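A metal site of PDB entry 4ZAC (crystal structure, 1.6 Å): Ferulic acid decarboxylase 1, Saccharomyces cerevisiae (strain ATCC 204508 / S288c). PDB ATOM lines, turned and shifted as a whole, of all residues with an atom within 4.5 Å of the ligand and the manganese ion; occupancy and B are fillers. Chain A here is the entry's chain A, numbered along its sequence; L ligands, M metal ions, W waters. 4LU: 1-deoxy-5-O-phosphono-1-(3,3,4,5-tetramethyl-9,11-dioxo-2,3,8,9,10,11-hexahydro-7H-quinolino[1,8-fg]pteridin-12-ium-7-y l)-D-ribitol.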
ATOM      1  N   GLN A 154      15.164  30.854  15.118  1.00  0.00           N
ATOM      2  CA  GLN A 154      15.463  31.115  13.696  1.00  0.00           C
ATOM      3  C   GLN A 154      14.938  29.936  12.818  1.00  0.00           C
ATOM      4  O   GLN A 154      15.602  28.867  12.637  1.00  0.00           O
ATOM      5  CB  GLN A 154      16.938  31.354  13.597  1.00  0.00           C
ATOM      6  CG  GLN A 154      17.685  31.212  12.250  1.00  0.00           C
ATOM      7  CD  GLN A 154      16.996  31.863  11.047  1.00  0.00           C
ATOM      8  OE1 GLN A 154      15.824  32.187  11.119  1.00  0.00           O
ATOM      9  NE2 GLN A 154      17.778  32.155   9.984  1.00  0.00           N
ATOM     10  N   THR A 155      13.696  30.166  12.317  1.00  0.00           N
ATOM     11  CA  THR A 155      13.223  29.281  11.266  1.00  0.00           C
ATOM     12  C   THR A 155      12.838  30.044  10.008  1.00  0.00           C
ATOM     13  O   THR A 155      12.576  29.414   8.993  1.00  0.00           O
ATOM     14  CB  THR A 155      11.994  28.506  11.722  1.00  0.00           C
ATOM     15  OG1 THR A 155      10.885  29.378  12.127  1.00  0.00           O
ATOM     16  CG2 THR A 155      12.340  27.611  12.992  1.00  0.00           C
ATOM     17  N   TYR A 156      12.656  31.379  10.094  1.00  0.00           N
ATOM     18  CA  TYR A 156      12.243  32.114   8.870  1.00  0.00           C
ATOM     19  C   TYR A 156      12.803  33.525   8.876  1.00  0.00           C
ATOM     20  O   TYR A 156      12.166  34.530   8.451  1.00  0.00           O
ATOM     21  CB  TYR A 156      10.714  32.105   8.792  1.00  0.00           C
ATOM     22  CG  TYR A 156      10.166  32.327   7.379  1.00  0.00           C
ATOM     23  CD1 TYR A 156      10.184  31.299   6.485  1.00  0.00           C
ATOM     24  CD2 TYR A 156       9.609  33.598   6.976  1.00  0.00           C
ATOM     25  CE1 TYR A 156       9.732  31.472   5.176  1.00  0.00           C
ATOM     26  CE2 TYR A 156       9.047  33.737   5.682  1.00  0.00           C
ATOM     27  CZ  TYR A 156       9.131  32.664   4.816  1.00  0.00           C
ATOM     28  OH  TYR A 156       8.606  32.686   3.539  1.00  0.00           O
ATOM     29  N   TRP A 168      31.277  39.812  -1.427  1.00  0.00           N
ATOM     30  CA  TRP A 168      30.079  38.838  -1.517  1.00  0.00           C
ATOM     31  C   TRP A 168      29.416  38.906  -0.190  1.00  0.00           C
ATOM     32  O   TRP A 168      29.989  38.597   0.888  1.00  0.00           O
ATOM     33  CB  TRP A 168      30.598  37.425  -1.846  1.00  0.00           C
ATOM     34  CG  TRP A 168      29.482  36.351  -1.860  1.00  0.00           C
ATOM     35  CD1 TRP A 168      28.132  36.577  -1.976  1.00  0.00           C
ATOM     36  CD2 TRP A 168      29.665  34.959  -1.740  1.00  0.00           C
ATOM     37  NE1 TRP A 168      27.455  35.328  -1.906  1.00  0.00           N
ATOM     38  CE2 TRP A 168      28.393  34.345  -1.780  1.00  0.00           C
ATOM     39  CE3 TRP A 168      30.825  34.167  -1.605  1.00  0.00           C
ATOM     40  CZ2 TRP A 168      28.225  32.941  -1.692  1.00  0.00           C
ATOM     41  CZ3 TRP A 168      30.707  32.792  -1.454  1.00  0.00           C
ATOM     42  CH2 TRP A 168      29.393  32.184  -1.519  1.00  0.00           C
ATOM     43  N   ASN A 170      26.199  37.284   1.637  1.00  0.00           N
ATOM     44  CA  ASN A 170      25.188  36.211   1.382  1.00  0.00           C
ATOM     45  C   ASN A 170      24.031  36.332   2.367  1.00  0.00           C
ATOM     46  O   ASN A 170      24.236  36.637   3.526  1.00  0.00           O
ATOM     47  CB  ASN A 170      25.883  34.835   1.614  1.00  0.00           C
ATOM     48  CG  ASN A 170      25.107  33.685   1.074  1.00  0.00           C
ATOM     49  OD1 ASN A 170      24.286  32.988   1.780  1.00  0.00           O
ATOM     50  ND2 ASN A 170      25.214  33.505  -0.172  1.00  0.00           N
ATOM     51  N   TRP A 171      22.819  36.164   1.860  1.00  0.00           N
ATOM     52  CA  TRP A 171      21.622  36.087   2.682  1.00  0.00           C
ATOM     53  C   TRP A 171      21.063  34.635   2.522  1.00  0.00           C
ATOM     54  O   TRP A 171      20.757  34.190   1.409  1.00  0.00           O
ATOM     55  CB  TRP A 171      20.576  37.054   2.103  1.00  0.00           C
ATOM     56  CG  TRP A 171      20.927  38.504   2.266  1.00  0.00           C
ATOM     57  CD1 TRP A 171      22.024  39.042   2.959  1.00  0.00           C
ATOM     58  CD2 TRP A 171      20.126  39.623   1.793  1.00  0.00           C
ATOM     59  NE1 TRP A 171      21.928  40.489   2.949  1.00  0.00           N
ATOM     60  CE2 TRP A 171      20.796  40.829   2.193  1.00  0.00           C
ATOM     61  CE3 TRP A 171      18.927  39.700   1.068  1.00  0.00           C
ATOM     62  CZ2 TRP A 171      20.228  42.165   1.968  1.00  0.00           C
ATOM     63  CZ3 TRP A 171      18.380  41.032   0.817  1.00  0.00           C
ATOM     64  CH2 TRP A 171      19.078  42.225   1.239  1.00  0.00           C
ATOM     65  N   SER A 172      20.816  34.009   3.656  1.00  0.00           N
ATOM     66  CA  SER A 172      20.311  32.615   3.661  1.00  0.00           C
ATOM     67  C   SER A 172      19.579  32.251   4.912  1.00  0.00           C
ATOM     68  O   SER A 172      19.667  32.877   5.933  1.00  0.00           O
ATOM     69  CB  SER A 172      21.504  31.628   3.352  1.00  0.00           C
ATOM     70  OG  SER A 172      22.301  31.681   4.475  1.00  0.00           O
ATOM     71  N   ILE A 173      18.707  31.263   4.757  1.00  0.00           N
ATOM     72  CA  ILE A 173      17.991  30.701   5.911  1.00  0.00           C
ATOM     73  C   ILE A 173      18.762  29.404   6.336  1.00  0.00           C
ATOM     74  O   ILE A 173      19.061  28.552   5.536  1.00  0.00           O
ATOM     75  CB  ILE A 173      16.564  30.335   5.561  1.00  0.00           C
ATOM     76  CG1 ILE A 173      15.849  31.607   4.992  1.00  0.00           C
ATOM     77  CG2 ILE A 173      15.780  29.839   6.851  1.00  0.00           C
ATOM     78  CD1 ILE A 173      14.304  31.237   4.714  1.00  0.00           C
ATOM     79  N   ALA A 174      19.015  29.327   7.640  1.00  0.00           N
ATOM     80  CA  ALA A 174      19.500  28.054   8.253  1.00  0.00           C
ATOM     81  C   ALA A 174      18.966  28.046   9.653  1.00  0.00           C
ATOM     82  O   ALA A 174      18.884  29.080  10.352  1.00  0.00           O
ATOM     83  CB  ALA A 174      21.020  28.047   8.319  1.00  0.00           C
ATOM     84  N   ARG A 175      18.573  26.882  10.134  1.00  0.00           N
ATOM     85  CA  ARG A 175      17.855  26.892  11.450  1.00  0.00           C
ATOM     86  C   ARG A 175      18.829  27.281  12.599  1.00  0.00           C
ATOM     87  O   ARG A 175      20.009  27.115  12.510  1.00  0.00           O
ATOM     88  CB  ARG A 175      17.362  25.505  11.799  1.00  0.00           C
ATOM     89  CG  ARG A 175      18.445  24.372  11.999  1.00  0.00           C
ATOM     90  CD  ARG A 175      17.759  23.086  12.068  1.00  0.00           C
ATOM     91  NE  ARG A 175      18.681  22.104  12.738  1.00  0.00           N
ATOM     92  CZ  ARG A 175      18.650  20.794  12.477  1.00  0.00           C
ATOM     93  NH1 ARG A 175      17.897  20.272  11.488  1.00  0.00           N
ATOM     94  NH2 ARG A 175      19.507  20.004  13.156  1.00  0.00           N
ATOM     95  N   LEU A 187      22.676  25.158  12.142  1.00  0.00           N
ATOM     96  CA  LEU A 187      23.395  24.436  11.079  1.00  0.00           C
ATOM     97  C   LEU A 187      24.258  25.410  10.247  1.00  0.00           C
ATOM     98  O   LEU A 187      23.771  26.478   9.745  1.00  0.00           O
ATOM     99  CB  LEU A 187      22.398  23.705  10.191  1.00  0.00           C
ATOM    100  CG  LEU A 187      21.749  22.474  10.829  1.00  0.00           C
ATOM    101  CD1 LEU A 187      20.717  21.860   9.830  1.00  0.00           C
ATOM    102  CD2 LEU A 187      22.779  21.372  11.203  1.00  0.00           C
ATOM    103  N   ILE A 189      26.593  24.230   7.474  1.00  0.00           N
ATOM    104  CA  ILE A 189      27.060  22.984   6.824  1.00  0.00           C
ATOM    105  C   ILE A 189      27.423  23.115   5.383  1.00  0.00           C
ATOM    106  O   ILE A 189      26.769  23.858   4.647  1.00  0.00           O
ATOM    107  CB  ILE A 189      26.057  21.808   6.985  1.00  0.00           C
ATOM    108  CG1 ILE A 189      24.742  22.065   6.174  1.00  0.00           C
ATOM    109  CG2 ILE A 189      25.841  21.532   8.472  1.00  0.00           C
ATOM    110  CD1 ILE A 189      23.821  20.782   5.865  1.00  0.00           C
ATOM    111  N   GLN A 192      26.537  24.663   1.881  1.00  0.00           N
ATOM    112  CA  GLN A 192      25.798  25.945   1.981  1.00  0.00           C
ATOM    113  C   GLN A 192      26.741  27.139   1.969  1.00  0.00           C
ATOM    114  O   GLN A 192      27.892  27.076   2.501  1.00  0.00           O
ATOM    115  CB  GLN A 192      24.936  25.984   3.241  1.00  0.00           C
ATOM    116  CG  GLN A 192      23.914  24.711   3.249  1.00  0.00           C
ATOM    117  CD  GLN A 192      22.953  24.817   2.124  1.00  0.00           C
ATOM    118  OE1 GLN A 192      23.262  24.771   0.887  1.00  0.00           O
ATOM    119  NE2 GLN A 192      21.685  25.097   2.517  1.00  0.00           N
ATOM    120  N   HIS A 193      26.229  28.283   1.457  1.00  0.00           N
ATOM    121  CA  HIS A 193      27.126  29.435   1.387  1.00  0.00           C
ATOM    122  C   HIS A 193      27.466  30.005   2.763  1.00  0.00           C
ATOM    123  O   HIS A 193      28.506  30.678   2.873  1.00  0.00           O
ATOM    124  CB  HIS A 193      26.549  30.495   0.435  1.00  0.00           C
ATOM    125  CG  HIS A 193      26.548  29.998  -0.985  1.00  0.00           C
ATOM    126  ND1 HIS A 193      25.723  30.554  -1.934  1.00  0.00           N
ATOM    127  CD2 HIS A 193      27.243  28.995  -1.585  1.00  0.00           C
ATOM    128  CE1 HIS A 193      25.934  29.927  -3.100  1.00  0.00           C
ATOM    129  NE2 HIS A 193      26.860  28.984  -2.909  1.00  0.00           N
ATOM    130  N   ILE A 194      26.607  29.880   3.735  1.00  0.00           N
ATOM    131  CA  ILE A 194      26.943  30.423   5.068  1.00  0.00           C
ATOM    132  C   ILE A 194      28.257  29.729   5.563  1.00  0.00           C
ATOM    133  O   ILE A 194      29.079  30.349   6.152  1.00  0.00           O
ATOM    134  CB  ILE A 194      25.736  30.229   6.026  1.00  0.00           C
ATOM    135  CG1 ILE A 194      26.050  30.957   7.336  1.00  0.00           C
ATOM    136  CG2 ILE A 194      25.461  28.636   6.199  1.00  0.00           C
ATOM    137  CD1 ILE A 194      24.709  30.953   8.243  1.00  0.00           C
ATOM    138  N   SER A 226      16.625  34.318   0.114  1.00  0.00           N
ATOM    139  CA  SER A 226      17.446  33.676   1.169  1.00  0.00           C
ATOM    140  C   SER A 226      17.346  32.144   1.072  1.00  0.00           C
ATOM    141  O   SER A 226      18.367  31.455   1.415  1.00  0.00           O
ATOM    142  CB  SER A 226      17.027  34.139   2.565  1.00  0.00           C
ATOM    143  OG  SER A 226      17.426  35.551   2.617  1.00  0.00           O
ATOM    144  N   SER A 227      16.190  31.585   0.665  1.00  0.00           N
ATOM    145  CA  SER A 227      15.986  30.154   0.590  1.00  0.00           C
ATOM    146  C   SER A 227      16.376  29.556  -0.772  1.00  0.00           C
ATOM    147  O   SER A 227      16.190  28.339  -1.026  1.00  0.00           O
ATOM    148  CB  SER A 227      14.539  29.784   0.833  1.00  0.00           C
ATOM    149  OG  SER A 227      14.354  28.388   0.805  1.00  0.00           O
ATOM    150  N   MET A 228      16.883  30.405  -1.668  1.00  0.00           N
ATOM    151  CA  MET A 228      17.154  29.964  -3.056  1.00  0.00           C
ATOM    152  C   MET A 228      18.661  29.744  -3.305  1.00  0.00           C
ATOM    153  O   MET A 228      19.474  30.590  -2.882  1.00  0.00           O
ATOM    154  CB  MET A 228      16.737  31.106  -3.993  1.00  0.00           C
ATOM    155  CG  MET A 228      16.803  30.644  -5.463  1.00  0.00           C
ATOM    156  SD  MET A 228      16.000  32.102  -6.375  1.00  0.00           S
ATOM    157  CE  MET A 228      15.976  31.394  -7.980  1.00  0.00           C
ATOM    158  N   PRO A 229      19.032  28.655  -3.964  1.00  0.00           N
ATOM    159  CA  PRO A 229      20.439  28.359  -4.190  1.00  0.00           C
ATOM    160  C   PRO A 229      20.933  29.056  -5.446  1.00  0.00           C
ATOM    161  O   PRO A 229      21.207  28.380  -6.439  1.00  0.00           O
ATOM    162  CB  PRO A 229      20.462  26.822  -4.251  1.00  0.00           C
ATOM    163  CG  PRO A 229      19.067  26.467  -4.944  1.00  0.00           C
ATOM    164  CD  PRO A 229      18.140  27.485  -4.260  1.00  0.00           C
ATOM    165  N   ILE A 230      21.067  30.383  -5.365  1.00  0.00           N
ATOM    166  CA  ILE A 230      21.647  31.111  -6.509  1.00  0.00           C
ATOM    167  C   ILE A 230      23.174  30.891  -6.471  1.00  0.00           C
ATOM    168  O   ILE A 230      23.704  30.319  -5.533  1.00  0.00           O
ATOM    169  CB  ILE A 230      21.270  32.609  -6.442  1.00  0.00           C
ATOM    170  CG1 ILE A 230      21.965  33.321  -5.269  1.00  0.00           C
ATOM    171  CG2 ILE A 230      19.761  32.741  -6.322  1.00  0.00           C
ATOM    172  CD1 ILE A 230      21.701  34.894  -5.369  1.00  0.00           C
ATOM    173  N   GLU A 236      22.749  37.921  -2.740  1.00  0.00           N
ATOM    174  CA  GLU A 236      21.274  37.782  -2.882  1.00  0.00           C
ATOM    175  C   GLU A 236      20.672  39.202  -3.013  1.00  0.00           C
ATOM    176  O   GLU A 236      19.710  39.373  -3.739  1.00  0.00           O
ATOM    177  CB  GLU A 236      20.654  37.085  -1.649  1.00  0.00           C
ATOM    178  CG  GLU A 236      20.789  35.482  -1.695  1.00  0.00           C
ATOM    179  CD  GLU A 236      22.201  34.938  -1.426  1.00  0.00           C
ATOM    180  OE1 GLU A 236      23.104  35.720  -0.983  1.00  0.00           O
ATOM    181  OE2 GLU A 236      22.322  33.696  -1.603  1.00  0.00           O
ATOM    182  N   PHE A 283      15.775  18.596  15.334  1.00  0.00           N
ATOM    183  CA  PHE A 283      14.709  19.532  15.000  1.00  0.00           C
ATOM    184  C   PHE A 283      13.799  18.850  14.002  1.00  0.00           C
ATOM    185  O   PHE A 283      14.301  18.133  13.117  1.00  0.00           O
ATOM    186  CB  PHE A 283      15.344  20.736  14.311  1.00  0.00           C
ATOM    187  CG  PHE A 283      14.313  21.836  13.972  1.00  0.00           C
ATOM    188  CD1 PHE A 283      13.463  22.383  14.968  1.00  0.00           C
ATOM    189  CD2 PHE A 283      14.223  22.306  12.610  1.00  0.00           C
ATOM    190  CE1 PHE A 283      12.466  23.402  14.617  1.00  0.00           C
ATOM    191  CE2 PHE A 283      13.274  23.328  12.302  1.00  0.00           C
ATOM    192  CZ  PHE A 283      12.409  23.847  13.247  1.00  0.00           C
ATOM    193  N   GLU A 285      12.017  18.128  10.936  1.00  0.00           N
ATOM    194  CA  GLU A 285      12.563  18.631   9.676  1.00  0.00           C
ATOM    195  C   GLU A 285      11.600  18.340   8.424  1.00  0.00           C
ATOM    196  O   GLU A 285      10.496  17.803   8.552  1.00  0.00           O
ATOM    197  CB  GLU A 285      13.906  17.996   9.510  1.00  0.00           C
ATOM    198  CG  GLU A 285      15.063  18.905   9.916  1.00  0.00           C
ATOM    199  CD  GLU A 285      15.171  20.229   9.069  1.00  0.00           C
ATOM    200  OE1 GLU A 285      14.432  20.425   7.983  1.00  0.00           O
ATOM    201  OE2 GLU A 285      16.068  21.123   9.477  1.00  0.00           O
ATOM    202  N   SER A 317       8.465  29.141  10.601  1.00  0.00           N
ATOM    203  CA  SER A 317       8.089  27.944   9.818  1.00  0.00           C
ATOM    204  C   SER A 317       8.317  26.710  10.777  1.00  0.00           C
ATOM    205  O   SER A 317       9.265  26.616  11.525  1.00  0.00           O
ATOM    206  CB  SER A 317       9.120  27.778   8.648  1.00  0.00           C
ATOM    207  OG  SER A 317       8.924  26.575   7.945  1.00  0.00           O
ATOM    208  N   PRO A 319       8.439  22.884  10.277  1.00  0.00           N
ATOM    209  CA  PRO A 319       8.508  21.861   9.201  1.00  0.00           C
ATOM    210  C   PRO A 319       7.981  20.538   9.653  1.00  0.00           C
ATOM    211  O   PRO A 319       8.002  20.147  10.841  1.00  0.00           O
ATOM    212  CB  PRO A 319      10.070  21.718   8.895  1.00  0.00           C
ATOM    213  CG  PRO A 319      10.646  23.024   9.456  1.00  0.00           C
ATOM    214  CD  PRO A 319       9.746  23.364  10.694  1.00  0.00           C
ATOM    215  N   GLU A 325       6.898  25.530   4.337  1.00  0.00           N
ATOM    216  CA  GLU A 325       7.905  26.273   3.599  1.00  0.00           C
ATOM    217  C   GLU A 325       9.064  25.406   3.107  1.00  0.00           C
ATOM    218  O   GLU A 325       9.777  25.805   2.218  1.00  0.00           O
ATOM    219  CB  GLU A 325       8.459  27.421   4.416  1.00  0.00           C
ATOM    220  CG  GLU A 325       7.423  28.527   4.849  1.00  0.00           C
ATOM    221  CD  GLU A 325       6.372  28.099   5.829  1.00  0.00           C
ATOM    222  OE1 GLU A 325       6.577  27.150   6.618  1.00  0.00           O
ATOM    223  OE2 GLU A 325       5.323  28.745   5.845  1.00  0.00           O
ATOM    224  N   THR A 326       9.333  24.303   3.844  1.00  0.00           N
ATOM    225  CA  THR A 326      10.482  23.481   3.389  1.00  0.00           C
ATOM    226  C   THR A 326      10.098  22.731   2.123  1.00  0.00           C
ATOM    227  O   THR A 326      10.953  22.078   1.557  1.00  0.00           O
ATOM    228  CB  THR A 326      10.951  22.517   4.486  1.00  0.00           C
ATOM    229  OG1 THR A 326       9.924  21.547   4.788  1.00  0.00           O
ATOM    230  CG2 THR A 326      11.297  23.261   5.731  1.00  0.00           C
ATOM    231  N   LEU A 329       9.098  26.507  -0.539  1.00  0.00           N
ATOM    232  CA  LEU A 329      10.211  27.385  -0.864  1.00  0.00           C
ATOM    233  C   LEU A 329      11.425  26.477  -1.139  1.00  0.00           C
ATOM    234  O   LEU A 329      12.004  26.570  -2.247  1.00  0.00           O
ATOM    235  CB  LEU A 329      10.575  28.342   0.239  1.00  0.00           C
ATOM    236  CG  LEU A 329       9.464  29.331   0.522  1.00  0.00           C
ATOM    237  CD1 LEU A 329       9.978  30.289   1.593  1.00  0.00           C
ATOM    238  CD2 LEU A 329       9.049  30.184  -0.729  1.00  0.00           C
ATOM    239  N   ILE A 330      11.825  25.549  -0.277  1.00  0.00           N
ATOM    240  CA  ILE A 330      13.077  24.893  -0.546  1.00  0.00           C
ATOM    241  C   ILE A 330      12.941  24.115  -1.881  1.00  0.00           C
ATOM    242  O   ILE A 330      13.753  24.219  -2.747  1.00  0.00           O
ATOM    243  CB  ILE A 330      13.448  23.899   0.583  1.00  0.00           C
ATOM    244  CG1 ILE A 330      13.752  24.751   1.853  1.00  0.00           C
ATOM    245  CG2 ILE A 330      14.831  23.168   0.234  1.00  0.00           C
ATOM    246  CD1 ILE A 330      14.119  23.831   3.025  1.00  0.00           C
ATOM    247  N   LYS A 394      25.596  21.565  -6.199  1.00  0.00           N
ATOM    248  CA  LYS A 394      24.930  21.995  -4.971  1.00  0.00           C
ATOM    249  C   LYS A 394      23.369  21.986  -5.228  1.00  0.00           C
ATOM    250  O   LYS A 394      22.626  21.698  -4.319  1.00  0.00           O
ATOM    251  CB  LYS A 394      25.396  23.427  -4.645  1.00  0.00           C
ATOM    252  CG  LYS A 394      24.628  24.063  -3.416  1.00  0.00           C
ATOM    253  CD  LYS A 394      25.469  25.308  -3.016  1.00  0.00           C
ATOM    254  CE  LYS A 394      24.793  26.148  -1.865  1.00  0.00           C
ATOM    255  NZ  LYS A 394      23.476  26.755  -2.371  1.00  0.00           N
HETATM  256  C9  4LU L   1      15.078  26.896   4.101  1.00  0.00           C
HETATM  257  C8  4LU L   1      13.833  27.200   4.662  1.00  0.00           C
HETATM  258  C7  4LU L   1      13.431  26.894   5.974  1.00  0.00           C
HETATM  259  C10 4LU L   1      18.152  25.366   5.307  1.00  0.00           C
HETATM  260  C6  4LU L   1      14.319  26.140   6.788  1.00  0.00           C
HETATM  261  N3  4LU L   1      20.141  24.712   7.037  1.00  0.00           N
HETATM  262  C2  4LU L   1      20.450  24.874   5.771  1.00  0.00           C
HETATM  263  C13 4LU L   1      12.593  25.793   8.682  1.00  0.00           C
HETATM  264  C5  4LU L   1      14.097  25.749   8.164  1.00  0.00           C
HETATM  265  C1  4LU L   1      16.002  24.586   8.141  1.00  0.00           C
HETATM  266  O2  4LU L   1      21.619  24.929   5.508  1.00  0.00           O
HETATM  267  N1  4LU L   1      19.472  25.259   4.876  1.00  0.00           N
HETATM  268  C4  4LU L   1      18.810  24.717   7.467  1.00  0.00           C
HETATM  269  O4  4LU L   1      18.721  24.539   8.678  1.00  0.00           O
HETATM  270  C4A 4LU L   1      17.785  25.082   6.620  1.00  0.00           C
HETATM  271  N5  4LU L   1      16.438  25.119   6.968  1.00  0.00           N
HETATM  272  C3  4LU L   1      14.555  24.316   8.237  1.00  0.00           C
HETATM  273  C12 4LU L   1      14.818  26.706   9.151  1.00  0.00           C
HETATM  274  C5A 4LU L   1      15.553  25.816   6.171  1.00  0.00           C
HETATM  275  C7M 4LU L   1      12.000  27.356   6.457  1.00  0.00           C
HETATM  276  C8M 4LU L   1      12.899  27.929   3.698  1.00  0.00           C
HETATM  277  C9A 4LU L   1      15.983  26.193   4.906  1.00  0.00           C
HETATM  278  N10 4LU L   1      17.237  25.741   4.410  1.00  0.00           N
HETATM  279  C1' 4LU L   1      17.520  25.935   2.995  1.00  0.00           C
HETATM  280  C2' 4LU L   1      18.440  27.080   2.511  1.00  0.00           C
HETATM  281  O2' 4LU L   1      17.904  28.302   2.995  1.00  0.00           O
HETATM  282  C3' 4LU L   1      18.771  26.970   1.104  1.00  0.00           C
HETATM  283  O3' 4LU L   1      19.392  25.717   0.741  1.00  0.00           O
HETATM  284  C4' 4LU L   1      19.404  28.212   0.488  1.00  0.00           C
HETATM  285  O4' 4LU L   1      19.712  27.919  -0.873  1.00  0.00           O
HETATM  286  C5' 4LU L   1      20.716  28.360   1.317  1.00  0.00           C
HETATM  287  O5' 4LU L   1      21.308  29.614   0.800  1.00  0.00           O
HETATM  288  P   4LU L   1      22.744  29.606   0.048  1.00  0.00           P
HETATM  289  O2P 4LU L   1      23.684  28.804   0.932  1.00  0.00           O
HETATM  290  O3P 4LU L   1      22.493  29.010  -1.293  1.00  0.00           O
HETATM  291  O1P 4LU L   1      23.117  31.070  -0.096  1.00  0.00           O
HETATM  292 MN    MN M   1      24.043  32.327  -1.684  1.00  0.00          MN
HETATM  293  O   HOH W   1      22.802  30.964  -3.076  1.00  0.00           O
HETATM  294  O   HOH W   2      21.740  27.693   4.786  1.00  0.00           O
HETATM  295  O   HOH W   3      18.138  24.306  -0.961  1.00  0.00           O
HETATM  296  O   HOH W   4      23.678  29.330   3.463  1.00  0.00           O
HETATM  297  O   HOH W   5      21.604  25.090  -1.169  1.00  0.00           O
HETATM  298  O   HOH W   6      23.907  25.403   7.073  1.00  0.00           O
HETATM  299  O   HOH W   7      25.073  33.357  -3.473  1.00  0.00           O
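The backbone nitrogen (N) of Pro 229 sits close to an oxygen (O4') of the ligand. O of Thr 155 touches C7M of the ligand, 3.3 Å away. CB of Ser 172 touches O5' of the ligand (3.3 Å). Ala 174 touches the ligand (CA to C4, 3.5 Å). Leu 187 touches the ligand. Ser 226 touches the ligand (O to O5', 3.5 Å). Ser 227 touches the ligand. Glu 285 touches the ligand. Ser 317 touches the ligand. Pro 319 touches the ligand. Ile 330 touches the ligand. Hydrophobic or aromatic side chains that line the ligand: Ile 173, Ala 174, Leu 187, His 193, Pro 229, Pro 319 and Ile 330. 19 residues have an atom within 4 Å of the ligand: Thr 155, Asn 170, Ser 172, Ile 173, Ala 174, Arg 175, Leu 187, Gln 192, His 193, Ser 226, Ser 227, Met 228, Pro 229, Glu 236, Glu 285, Ser 317, Pro 319, Ile 330 and Lys 394. The nearest printed residue that does not touch the ligand is Glu 325 (4.1 Å).
The backbone carbonyl oxygen (O) of Met 228 sits close to an oxygen (O4') of the ligand (3.4 Å). N of His 193 lies within hydrogen-bond range of O2P of the ligand. N of Arg 175 sits at hydrogen-bond distance from O4 of the ligand. The side-chain amide nitrogen (NE2) of Gln 192 lies within hydrogen-bond range of an oxygen (O3') of the ligand (3.0 Å). NZ of Lys 394 is in salt-bridge range of O3P of the ligand. O2' of the ligand sits at hydrogen-bond distance from O of Ile 173, at 2.8 Å.
Water W1 lies within hydrogen-bond range of O3P of the ligand (2.7 Å), O of Ile 230 (2.7 Å) and O of Met 228 (3.4 Å). Water W4 lies within hydrogen-bond range of an oxygen (O2P) of the ligand (2.6 Å), the side-chain hydroxyl (OG) of Ser 172 (2.9 Å), the backbone NH (N) of Ile 194 (3.0 Å) and the backbone NH (N) of His 193 (3.4 Å). Water W6 lies within hydrogen-bond range of an oxygen (O2) of the ligand (2.8 Å), the backbone carbonyl oxygen (O) of Leu 187 (2.9 Å) and the backbone NH (N) of Ile 189 (3.0 Å). Water W2 lies within hydrogen-bond range of O2 of the ligand (2.9 Å), O of Ile 173 (2.9 Å) and NE2 of Gln 192 (3.4 Å). Water W5 lies within hydrogen-bond range of OE1 of Gln 192 (2.7 Å), NZ of Lys 394 (2.8 Å) and O3' of the ligand (3.0 Å).
The backbone NH (N) of Ser 317 sits at hydrogen-bond distance from the side-chain hydroxyl (OG1) of Thr 155 (2.9 Å). The guanidinium group (NH1) of Arg 175 is in salt-bridge range of the side-chain carboxylate (OE2) of Glu 285, 2.8 Å away. ND2 of Asn 170 lies close to NE1 of Trp 168, at 3.4 Å. The backbone carbonyl oxygen (O) of Ser 226 is in hydrogen-bond range of the backbone NH (N) of Ile 173, at 3.4 Å. The side-chain carboxylate of Glu 325 sits at hydrogen-bond distance from the side-chain hydroxyl of Ser 317, 2.8 Å away. O of Ala 174 lies close to NE2 of Gln 154, 3.3 Å away. N of Ile 330 lies within hydrogen-bond range of O of Glu 325. The backbone carbonyl oxygen (O) of Arg 175 sits at hydrogen-bond distance from the backbone NH (N) of Leu 187 (3.3 Å).
Of the 30 residues printed, 3 come within 4 Å of the manganese ion.
The manganese ion is bound by OE2 of Glu 236 (2.2 Å), O1P of the ligand (2.2 Å), ND2 of Asn 170 (2.2 Å), water W7 (2.3 Å), water W1 (2.3 Å) and ND1 of His 193 (2.5 Å).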
